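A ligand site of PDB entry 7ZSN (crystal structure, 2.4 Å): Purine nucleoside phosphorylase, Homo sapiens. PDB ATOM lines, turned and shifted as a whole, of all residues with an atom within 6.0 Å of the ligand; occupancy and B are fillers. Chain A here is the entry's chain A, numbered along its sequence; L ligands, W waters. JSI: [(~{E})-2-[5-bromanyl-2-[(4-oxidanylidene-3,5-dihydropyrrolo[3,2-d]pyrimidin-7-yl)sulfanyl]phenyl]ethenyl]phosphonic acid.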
ATOM      1  N   CYS A  31      34.953  19.082   6.861  1.00  0.00           N
ATOM      2  CA  CYS A  31      34.041  20.213   7.170  1.00  0.00           C
ATOM      3  C   CYS A  31      33.205  20.545   5.934  1.00  0.00           C
ATOM      4  O   CYS A  31      33.789  20.762   4.846  1.00  0.00           O
ATOM      5  CB  CYS A  31      34.832  21.414   7.636  1.00  0.00           C
ATOM      6  SG  CYS A  31      36.094  20.969   8.860  1.00  0.00           S
ATOM      7  N   GLY A  32      31.883  20.555   6.104  1.00  0.00           N
ATOM      8  CA  GLY A  32      30.917  21.047   5.104  1.00  0.00           C
ATOM      9  C   GLY A  32      30.973  22.567   5.031  1.00  0.00           C
ATOM     10  O   GLY A  32      31.596  23.152   5.930  1.00  0.00           O
ATOM     11  N   SER A  33      30.368  23.162   3.988  1.00  0.00           N
ATOM     12  CA  SER A  33      30.271  24.627   3.785  1.00  0.00           C
ATOM     13  C   SER A  33      29.690  25.269   5.044  1.00  0.00           C
ATOM     14  O   SER A  33      28.538  24.924   5.397  1.00  0.00           O
ATOM     15  CB  SER A  33      29.433  24.962   2.566  1.00  0.00           C
ATOM     16  OG  SER A  33      30.077  24.545   1.366  1.00  0.00           O
ATOM     17  N   ARG A  84      36.269  21.071   0.628  1.00  0.00           N
ATOM     18  CA  ARG A  84      36.158  19.675   0.147  1.00  0.00           C
ATOM     19  C   ARG A  84      35.816  19.737  -1.347  1.00  0.00           C
ATOM     20  O   ARG A  84      35.308  20.782  -1.788  1.00  0.00           O
ATOM     21  CB  ARG A  84      35.116  18.954   1.012  1.00  0.00           C
ATOM     22  CG  ARG A  84      33.690  19.361   0.709  1.00  0.00           C
ATOM     23  CD  ARG A  84      32.837  18.127   0.673  1.00  0.00           C
ATOM     24  NE  ARG A  84      31.944  18.135   1.813  1.00  0.00           N
ATOM     25  CZ  ARG A  84      31.590  17.069   2.501  1.00  0.00           C
ATOM     26  NH1 ARG A  84      30.745  17.213   3.496  1.00  0.00           N
ATOM     27  NH2 ARG A  84      32.068  15.870   2.196  1.00  0.00           N
ATOM     28  N   HIS A  86      33.695  18.491  -4.772  1.00  0.00           N
ATOM     29  CA  HIS A  86      32.326  18.100  -5.202  1.00  0.00           C
ATOM     30  C   HIS A  86      32.363  17.707  -6.691  1.00  0.00           C
ATOM     31  O   HIS A  86      33.161  18.296  -7.432  1.00  0.00           O
ATOM     32  CB  HIS A  86      31.335  19.253  -5.033  1.00  0.00           C
ATOM     33  CG  HIS A  86      31.350  19.879  -3.695  1.00  0.00           C
ATOM     34  ND1 HIS A  86      32.300  20.787  -3.325  1.00  0.00           N
ATOM     35  CD2 HIS A  86      30.518  19.749  -2.634  1.00  0.00           C
ATOM     36  CE1 HIS A  86      32.064  21.196  -2.094  1.00  0.00           C
ATOM     37  NE2 HIS A  86      30.965  20.577  -1.646  1.00  0.00           N
ATOM     38  N   TYR A  88      30.085  18.414  -8.888  1.00  0.00           N
ATOM     39  CA  TYR A  88      29.603  19.576  -9.693  1.00  0.00           C
ATOM     40  C   TYR A  88      30.765  20.519 -10.071  1.00  0.00           C
ATOM     41  O   TYR A  88      30.559  21.331 -10.965  1.00  0.00           O
ATOM     42  CB  TYR A  88      28.490  20.365  -8.991  1.00  0.00           C
ATOM     43  CG  TYR A  88      28.876  21.063  -7.708  1.00  0.00           C
ATOM     44  CD1 TYR A  88      29.728  22.160  -7.696  1.00  0.00           C
ATOM     45  CD2 TYR A  88      28.374  20.622  -6.497  1.00  0.00           C
ATOM     46  CE1 TYR A  88      30.075  22.780  -6.509  1.00  0.00           C
ATOM     47  CE2 TYR A  88      28.702  21.231  -5.306  1.00  0.00           C
ATOM     48  CZ  TYR A  88      29.560  22.312  -5.308  1.00  0.00           C
ATOM     49  OH  TYR A  88      29.869  22.901  -4.118  1.00  0.00           O
ATOM     50  N   THR A 114      30.799  16.192   7.608  1.00  0.00           N
ATOM     51  CA  THR A 114      29.665  17.129   7.764  1.00  0.00           C
ATOM     52  C   THR A 114      29.370  17.737   6.404  1.00  0.00           C
ATOM     53  O   THR A 114      30.268  17.753   5.580  1.00  0.00           O
ATOM     54  CB  THR A 114      29.934  18.199   8.840  1.00  0.00           C
ATOM     55  OG1 THR A 114      30.875  19.136   8.327  1.00  0.00           O
ATOM     56  CG2 THR A 114      30.452  17.592  10.124  1.00  0.00           C
ATOM     57  N   ASN A 115      28.151  18.224   6.213  1.00  0.00           N
ATOM     58  CA  ASN A 115      27.688  18.864   4.957  1.00  0.00           C
ATOM     59  C   ASN A 115      26.563  19.836   5.310  1.00  0.00           C
ATOM     60  O   ASN A 115      26.065  19.782   6.439  1.00  0.00           O
ATOM     61  CB  ASN A 115      27.255  17.826   3.927  1.00  0.00           C
ATOM     62  CG  ASN A 115      26.075  16.969   4.362  1.00  0.00           C
ATOM     63  OD1 ASN A 115      24.980  17.466   4.620  1.00  0.00           O
ATOM     64  ND2 ASN A 115      26.272  15.668   4.379  1.00  0.00           N
ATOM     65  N   ALA A 116      26.219  20.716   4.374  1.00  0.00           N
ATOM     66  CA  ALA A 116      24.959  21.466   4.362  1.00  0.00           C
ATOM     67  C   ALA A 116      23.981  20.693   3.470  1.00  0.00           C
ATOM     68  O   ALA A 116      24.450  19.940   2.608  1.00  0.00           O
ATOM     69  CB  ALA A 116      25.185  22.871   3.865  1.00  0.00           C
ATOM     70  N   ALA A 117      22.685  20.832   3.711  1.00  0.00           N
ATOM     71  CA  ALA A 117      21.661  20.029   3.022  1.00  0.00           C
ATOM     72  C   ALA A 117      20.327  20.749   3.119  1.00  0.00           C
ATOM     73  O   ALA A 117      20.142  21.516   4.066  1.00  0.00           O
ATOM     74  CB  ALA A 117      21.579  18.666   3.631  1.00  0.00           C
ATOM     75  N   GLY A 118      19.474  20.532   2.126  1.00  0.00           N
ATOM     76  CA  GLY A 118      18.093  21.035   2.066  1.00  0.00           C
ATOM     77  C   GLY A 118      17.174  20.059   2.758  1.00  0.00           C
ATOM     78  O   GLY A 118      17.362  18.846   2.550  1.00  0.00           O
ATOM     79  N   GLY A 119      16.260  20.578   3.572  1.00  0.00           N
ATOM     80  CA  GLY A 119      15.261  19.760   4.273  1.00  0.00           C
ATOM     81  C   GLY A 119      14.160  19.331   3.325  1.00  0.00           C
ATOM     82  O   GLY A 119      13.599  20.189   2.640  1.00  0.00           O
ATOM     83  N   TYR A 192      20.174  10.859   4.015  1.00  0.00           N
ATOM     84  CA  TYR A 192      20.738  11.884   3.106  1.00  0.00           C
ATOM     85  C   TYR A 192      20.739  11.316   1.687  1.00  0.00           C
ATOM     86  O   TYR A 192      21.269  10.211   1.467  1.00  0.00           O
ATOM     87  CB  TYR A 192      22.148  12.245   3.559  1.00  0.00           C
ATOM     88  CG  TYR A 192      22.913  13.210   2.684  1.00  0.00           C
ATOM     89  CD1 TYR A 192      22.878  14.569   2.946  1.00  0.00           C
ATOM     90  CD2 TYR A 192      23.728  12.757   1.663  1.00  0.00           C
ATOM     91  CE1 TYR A 192      23.637  15.465   2.208  1.00  0.00           C
ATOM     92  CE2 TYR A 192      24.480  13.642   0.908  1.00  0.00           C
ATOM     93  CZ  TYR A 192      24.440  14.994   1.182  1.00  0.00           C
ATOM     94  OH  TYR A 192      25.180  15.879   0.448  1.00  0.00           O
ATOM     95  N   VAL A 195      22.539  14.191  -4.643  1.00  0.00           N
ATOM     96  CA  VAL A 195      22.361  14.566  -6.073  1.00  0.00           C
ATOM     97  C   VAL A 195      23.649  15.267  -6.508  1.00  0.00           C
ATOM     98  O   VAL A 195      24.386  15.781  -5.634  1.00  0.00           O
ATOM     99  CB  VAL A 195      21.138  15.474  -6.264  1.00  0.00           C
ATOM    100  CG1 VAL A 195      19.856  14.750  -5.891  1.00  0.00           C
ATOM    101  CG2 VAL A 195      21.268  16.782  -5.499  1.00  0.00           C
ATOM    102  N   SER A 199      22.832  22.857  -9.836  1.00  0.00           N
ATOM    103  CA  SER A 199      21.555  23.612  -9.793  1.00  0.00           C
ATOM    104  C   SER A 199      20.678  23.019  -8.688  1.00  0.00           C
ATOM    105  O   SER A 199      20.875  21.838  -8.357  1.00  0.00           O
ATOM    106  CB  SER A 199      20.882  23.619 -11.151  1.00  0.00           C
ATOM    107  OG  SER A 199      20.598  22.303 -11.587  1.00  0.00           O
ATOM    108  N   PHE A 200      19.784  23.814  -8.111  1.00  0.00           N
ATOM    109  CA  PHE A 200      18.835  23.373  -7.048  1.00  0.00           C
ATOM    110  C   PHE A 200      17.638  22.679  -7.702  1.00  0.00           C
ATOM    111  O   PHE A 200      17.382  22.855  -8.913  1.00  0.00           O
ATOM    112  CB  PHE A 200      18.419  24.539  -6.146  1.00  0.00           C
ATOM    113  CG  PHE A 200      19.484  25.075  -5.211  1.00  0.00           C
ATOM    114  CD1 PHE A 200      20.055  24.277  -4.231  1.00  0.00           C
ATOM    115  CD2 PHE A 200      19.881  26.406  -5.265  1.00  0.00           C
ATOM    116  CE1 PHE A 200      21.002  24.772  -3.357  1.00  0.00           C
ATOM    117  CE2 PHE A 200      20.829  26.910  -4.386  1.00  0.00           C
ATOM    118  CZ  PHE A 200      21.401  26.092  -3.433  1.00  0.00           C
ATOM    119  N   GLU A 201      16.890  21.929  -6.898  1.00  0.00           N
ATOM    120  CA  GLU A 201      15.815  21.019  -7.352  1.00  0.00           C
ATOM    121  C   GLU A 201      14.575  21.812  -7.761  1.00  0.00           C
ATOM    122  O   GLU A 201      14.302  22.857  -7.145  1.00  0.00           O
ATOM    123  CB  GLU A 201      15.431  20.037  -6.243  1.00  0.00           C
ATOM    124  CG  GLU A 201      16.531  19.037  -5.925  1.00  0.00           C
ATOM    125  CD  GLU A 201      17.665  19.577  -5.074  1.00  0.00           C
ATOM    126  OE1 GLU A 201      17.504  20.660  -4.492  1.00  0.00           O
ATOM    127  OE2 GLU A 201      18.703  18.905  -5.001  1.00  0.00           O
ATOM    128  N   VAL A 217      18.825  16.487   1.292  1.00  0.00           N
ATOM    129  CA  VAL A 217      19.497  16.375  -0.036  1.00  0.00           C
ATOM    130  C   VAL A 217      20.679  17.336  -0.071  1.00  0.00           C
ATOM    131  O   VAL A 217      20.505  18.511   0.280  1.00  0.00           O
ATOM    132  CB  VAL A 217      18.512  16.654  -1.182  1.00  0.00           C
ATOM    133  CG1 VAL A 217      17.842  17.998  -1.038  1.00  0.00           C
ATOM    134  CG2 VAL A 217      19.209  16.538  -2.529  1.00  0.00           C
ATOM    135  N   GLY A 218      21.843  16.836  -0.500  1.00  0.00           N
ATOM    136  CA  GLY A 218      23.054  17.655  -0.720  1.00  0.00           C
ATOM    137  C   GLY A 218      23.879  17.088  -1.866  1.00  0.00           C
ATOM    138  O   GLY A 218      23.439  16.080  -2.430  1.00  0.00           O
ATOM    139  N   MET A 219      25.039  17.661  -2.152  1.00  0.00           N
ATOM    140  CA  MET A 219      25.846  17.373  -3.371  1.00  0.00           C
ATOM    141  C   MET A 219      27.222  16.825  -2.994  1.00  0.00           C
ATOM    142  O   MET A 219      28.134  16.975  -3.832  1.00  0.00           O
ATOM    143  CB  MET A 219      25.984  18.648  -4.202  1.00  0.00           C
ATOM    144  CG  MET A 219      24.653  19.309  -4.503  1.00  0.00           C
ATOM    145  SD  MET A 219      24.822  20.966  -5.177  1.00  0.00           S
ATOM    146  CE  MET A 219      23.106  21.436  -5.357  1.00  0.00           C
ATOM    147  N   SER A 220      27.356  16.155  -1.847  1.00  0.00           N
ATOM    148  CA  SER A 220      28.653  15.697  -1.287  1.00  0.00           C
ATOM    149  C   SER A 220      28.506  14.402  -0.479  1.00  0.00           C
ATOM    150  O   SER A 220      27.459  13.760  -0.561  1.00  0.00           O
ATOM    151  CB  SER A 220      29.219  16.800  -0.438  1.00  0.00           C
ATOM    152  OG  SER A 220      28.407  17.007   0.702  1.00  0.00           O
ATOM    153  N   THR A 221      29.579  14.032   0.246  1.00  0.00           N
ATOM    154  CA  THR A 221      29.595  13.178   1.456  1.00  0.00           C
ATOM    155  C   THR A 221      29.548  11.695   1.067  1.00  0.00           C
ATOM    156  O   THR A 221      30.415  10.911   1.533  1.00  0.00           O
ATOM    157  CB  THR A 221      28.432  13.550   2.401  1.00  0.00           C
ATOM    158  OG1 THR A 221      28.596  14.918   2.759  1.00  0.00           O
ATOM    159  CG2 THR A 221      28.374  12.698   3.647  1.00  0.00           C
ATOM    160  N   THR A 242      20.107  23.893   5.957  1.00  0.00           N
ATOM    161  CA  THR A 242      20.309  25.336   5.640  1.00  0.00           C
ATOM    162  C   THR A 242      19.055  25.962   5.002  1.00  0.00           C
ATOM    163  O   THR A 242      19.002  27.191   4.912  1.00  0.00           O
ATOM    164  CB  THR A 242      21.522  25.500   4.724  1.00  0.00           C
ATOM    165  OG1 THR A 242      21.305  24.650   3.599  1.00  0.00           O
ATOM    166  CG2 THR A 242      22.819  25.159   5.405  1.00  0.00           C
ATOM    167  N   ASN A 243      18.085  25.154   4.605  1.00  0.00           N
ATOM    168  CA  ASN A 243      16.950  25.639   3.780  1.00  0.00           C
ATOM    169  C   ASN A 243      15.910  24.521   3.710  1.00  0.00           C
ATOM    170  O   ASN A 243      16.289  23.355   3.851  1.00  0.00           O
ATOM    171  CB  ASN A 243      17.430  26.107   2.408  1.00  0.00           C
ATOM    172  CG  ASN A 243      18.099  25.026   1.577  1.00  0.00           C
ATOM    173  OD1 ASN A 243      19.235  24.628   1.856  1.00  0.00           O
ATOM    174  ND2 ASN A 243      17.406  24.544   0.560  1.00  0.00           N
ATOM    175  N   VAL A 245      13.183  22.684   1.339  1.00  0.00           N
ATOM    176  CA  VAL A 245      13.154  22.506  -0.140  1.00  0.00           C
ATOM    177  C   VAL A 245      11.722  22.804  -0.595  1.00  0.00           C
ATOM    178  O   VAL A 245      10.785  22.152  -0.111  1.00  0.00           O
ATOM    179  CB  VAL A 245      13.631  21.103  -0.555  1.00  0.00           C
ATOM    180  CG1 VAL A 245      13.472  20.864  -2.059  1.00  0.00           C
ATOM    181  CG2 VAL A 245      15.077  20.852  -0.145  1.00  0.00           C
ATOM    182  N   ALA A 255      15.396  28.669  -3.402  1.00  0.00           N
ATOM    183  CA  ALA A 255      16.675  28.306  -2.739  1.00  0.00           C
ATOM    184  C   ALA A 255      17.786  29.187  -3.319  1.00  0.00           C
ATOM    185  O   ALA A 255      17.709  29.494  -4.518  1.00  0.00           O
ATOM    186  CB  ALA A 255      16.979  26.838  -2.921  1.00  0.00           C
ATOM    187  N   ASN A 256      18.765  29.593  -2.499  1.00  0.00           N
ATOM    188  CA  ASN A 256      19.858  30.526  -2.923  1.00  0.00           C
ATOM    189  C   ASN A 256      21.146  30.190  -2.150  1.00  0.00           C
ATOM    190  O   ASN A 256      21.037  29.691  -1.016  1.00  0.00           O
ATOM    191  CB  ASN A 256      19.486  32.003  -2.759  1.00  0.00           C
ATOM    192  CG  ASN A 256      18.661  32.318  -1.522  1.00  0.00           C
ATOM    193  OD1 ASN A 256      19.141  33.007  -0.624  1.00  0.00           O
ATOM    194  ND2 ASN A 256      17.427  31.827  -1.477  1.00  0.00           N
ATOM    195  N   HIS A 257      22.289  30.474  -2.774  1.00  0.00           N
ATOM    196  CA  HIS A 257      23.660  30.312  -2.198  1.00  0.00           C
ATOM    197  C   HIS A 257      23.763  31.110  -0.896  1.00  0.00           C
ATOM    198  O   HIS A 257      24.274  30.540   0.087  1.00  0.00           O
ATOM    199  CB  HIS A 257      24.733  30.708  -3.236  1.00  0.00           C
ATOM    200  N   VAL A 260      22.062  29.687   2.301  1.00  0.00           N
ATOM    201  CA  VAL A 260      22.835  28.480   2.733  1.00  0.00           C
ATOM    202  C   VAL A 260      24.025  28.965   3.565  1.00  0.00           C
ATOM    203  O   VAL A 260      24.178  28.475   4.699  1.00  0.00           O
ATOM    204  CB  VAL A 260      23.266  27.596   1.545  1.00  0.00           C
ATOM    205  CG1 VAL A 260      24.105  26.402   1.999  1.00  0.00           C
ATOM    206  CG2 VAL A 260      22.074  27.113   0.731  1.00  0.00           C
ATOM    207  N   LEU A 261      24.823  29.896   3.018  1.00  0.00           N
ATOM    208  CA  LEU A 261      25.992  30.526   3.687  1.00  0.00           C
ATOM    209  C   LEU A 261      25.560  31.146   5.025  1.00  0.00           C
ATOM    210  O   LEU A 261      26.247  30.900   6.032  1.00  0.00           O
ATOM    211  CB  LEU A 261      26.605  31.593   2.775  1.00  0.00           C
ATOM    212  CG  LEU A 261      27.270  31.089   1.501  1.00  0.00           C
ATOM    213  CD1 LEU A 261      27.850  32.264   0.712  1.00  0.00           C
ATOM    214  CD2 LEU A 261      28.353  30.067   1.801  1.00  0.00           C
HETATM  215  N1  JSI L   1      19.405  20.991  -2.537  1.00  0.00           N
HETATM  216  N3  JSI L   1      20.888  23.002   0.161  1.00  0.00           N
HETATM  217  C4  JSI L   1      20.524  22.194  -0.881  1.00  0.00           C
HETATM  218  C5  JSI L   1      22.734  21.996  -0.549  1.00  0.00           C
HETATM  219  C6  JSI L   1      22.237  22.904   0.354  1.00  0.00           C
HETATM  220  C7  JSI L   1      25.140  23.177  -0.823  1.00  0.00           C
HETATM  221  C8  JSI L   1      26.374  23.428  -0.220  1.00  0.00           C
HETATM  222  C10 JSI L   1      26.191  25.741  -0.848  1.00  0.00           C
HETATM  223  C13 JSI L   1      27.113  22.375   0.477  1.00  0.00           C
HETATM  224  C1  JSI L   1      19.274  21.921  -1.501  1.00  0.00           C
HETATM  225  C2  JSI L   1      20.549  20.419  -2.919  1.00  0.00           C
HETATM  226  N2  JSI L   1      21.693  20.671  -2.355  1.00  0.00           N
HETATM  227  C3  JSI L   1      21.679  21.555  -1.330  1.00  0.00           C
HETATM  228  S1  JSI L   1      24.415  21.554  -0.767  1.00  0.00           S
HETATM  229  C9  JSI L   1      26.889  24.730  -0.234  1.00  0.00           C
HETATM  230  C11 JSI L   1      24.976  25.501  -1.455  1.00  0.00           C
HETATM  231  C12 JSI L   1      24.458  24.222  -1.439  1.00  0.00           C
HETATM  232 BR1  JSI L   1      26.901  27.495  -0.846  1.00  0.00          BR
HETATM  233  C14 JSI L   1      28.361  21.991   0.306  1.00  0.00           C
HETATM  234  P1  JSI L   1      28.939  20.718   1.317  1.00  0.00           P
HETATM  235  O1  JSI L   1      30.400  20.500   1.189  1.00  0.00           O
HETATM  236  O2  JSI L   1      28.244  19.426   1.000  1.00  0.00           O
HETATM  237  O3  JSI L   1      28.629  21.064   2.732  1.00  0.00           O
HETATM  238  O4  JSI L   1      18.171  22.405  -1.220  1.00  0.00           O
HETATM  239  O   HOH W   1      25.853  18.499   0.997  1.00  0.00           O
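Water W1 lies within hydrogen-bond range of O2 of the ligand (2.6 Å), O of Ala 116 (2.6 Å), OH of Tyr 192 (2.8 Å), OG of Ser 220 (3.0 Å) and N of Met 219 (3.4 Å).
The side-chain hydroxyl (OG) of Ser 220 is in hydrogen-bond range of an oxygen (O2) of the ligand (2.4 Å).
The side-chain amide oxygen (OD1) of Asn 243 lies within hydrogen-bond range of a nitrogen (N3) of the ligand, 2.9 Å away.
The side-chain carboxylate (OE1) of Glu 201 lies within hydrogen-bond range of a nitrogen (N1) of the ligand, at 2.7 Å.
An oxygen (O3) of the ligand sits at hydrogen-bond distance from the backbone NH (N) of Ala 116 (2.9 Å).
The backbone NH (N) of Ser 33 sits at hydrogen-bond distance from an oxygen (O3) of the ligand (3.0 Å).
NE2 of His 86 is in hydrogen-bond range of O1 of the ligand (2.9 Å).
The guanidinium group (NE) of Arg 84 lies within salt-bridge range of an oxygen (O1) of the ligand (2.9 Å).
N3 of the ligand lies close to N of Gly 118, 3.5 Å away.
The backbone NH (N) of Ser 220 sits at hydrogen-bond distance from the side-chain hydroxyl (OH) of Tyr 192, 3.2 Å away.
O of Gly 218 lies within hydrogen-bond range of N of Val 195, at 3.0 Å.
OH of Tyr 192 lies close to O of Gly 218.
The side-chain hydroxyl (OG1) of Thr 114 is in hydrogen-bond range of the backbone NH (N) of Gly 32.
The backbone carbonyl oxygen of Val 217 is in hydrogen-bond range of the backbone NH of Gly 118 (2.9 Å).
The side-chain hydroxyl (OG1) of Thr 221 lies within hydrogen-bond range of the side-chain amide nitrogen (ND2) of Asn 115, 2.9 Å away.
OG of Ser 220 is in hydrogen-bond range of OG1 of Thr 221, 2.9 Å away.
The backbone carbonyl oxygen (O) of Asn 243 is in hydrogen-bond range of the backbone NH (N) of Gly 119, at 2.8 Å.
Gly 32 touches the ligand (CA to O3, 3.3 Å).
Asn 115 touches the ligand.
Ala 117 touches the ligand (C to N3, 3.8 Å).
CE1 of Phe 200 touches C4 of the ligand (3.6 Å).
O of Val 217 touches N2 of the ligand (3.6 Å).
Gly 218 touches the ligand (CA to N2, 3.7 Å).
CE of Met 219 touches N2 of the ligand, at 3.4 Å.
Thr 242 touches the ligand.
CG2 of Val 245 touches O4 of the ligand, 3.6 Å away.
Val 260 touches the ligand (CG1 to C10, 3.6 Å).
Leu 261 touches the ligand.
Of the 30 residues printed, 19 come within 4 Å of the ligand.
The nearest printed residue that does not touch the ligand is His 257 (4.1 Å).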
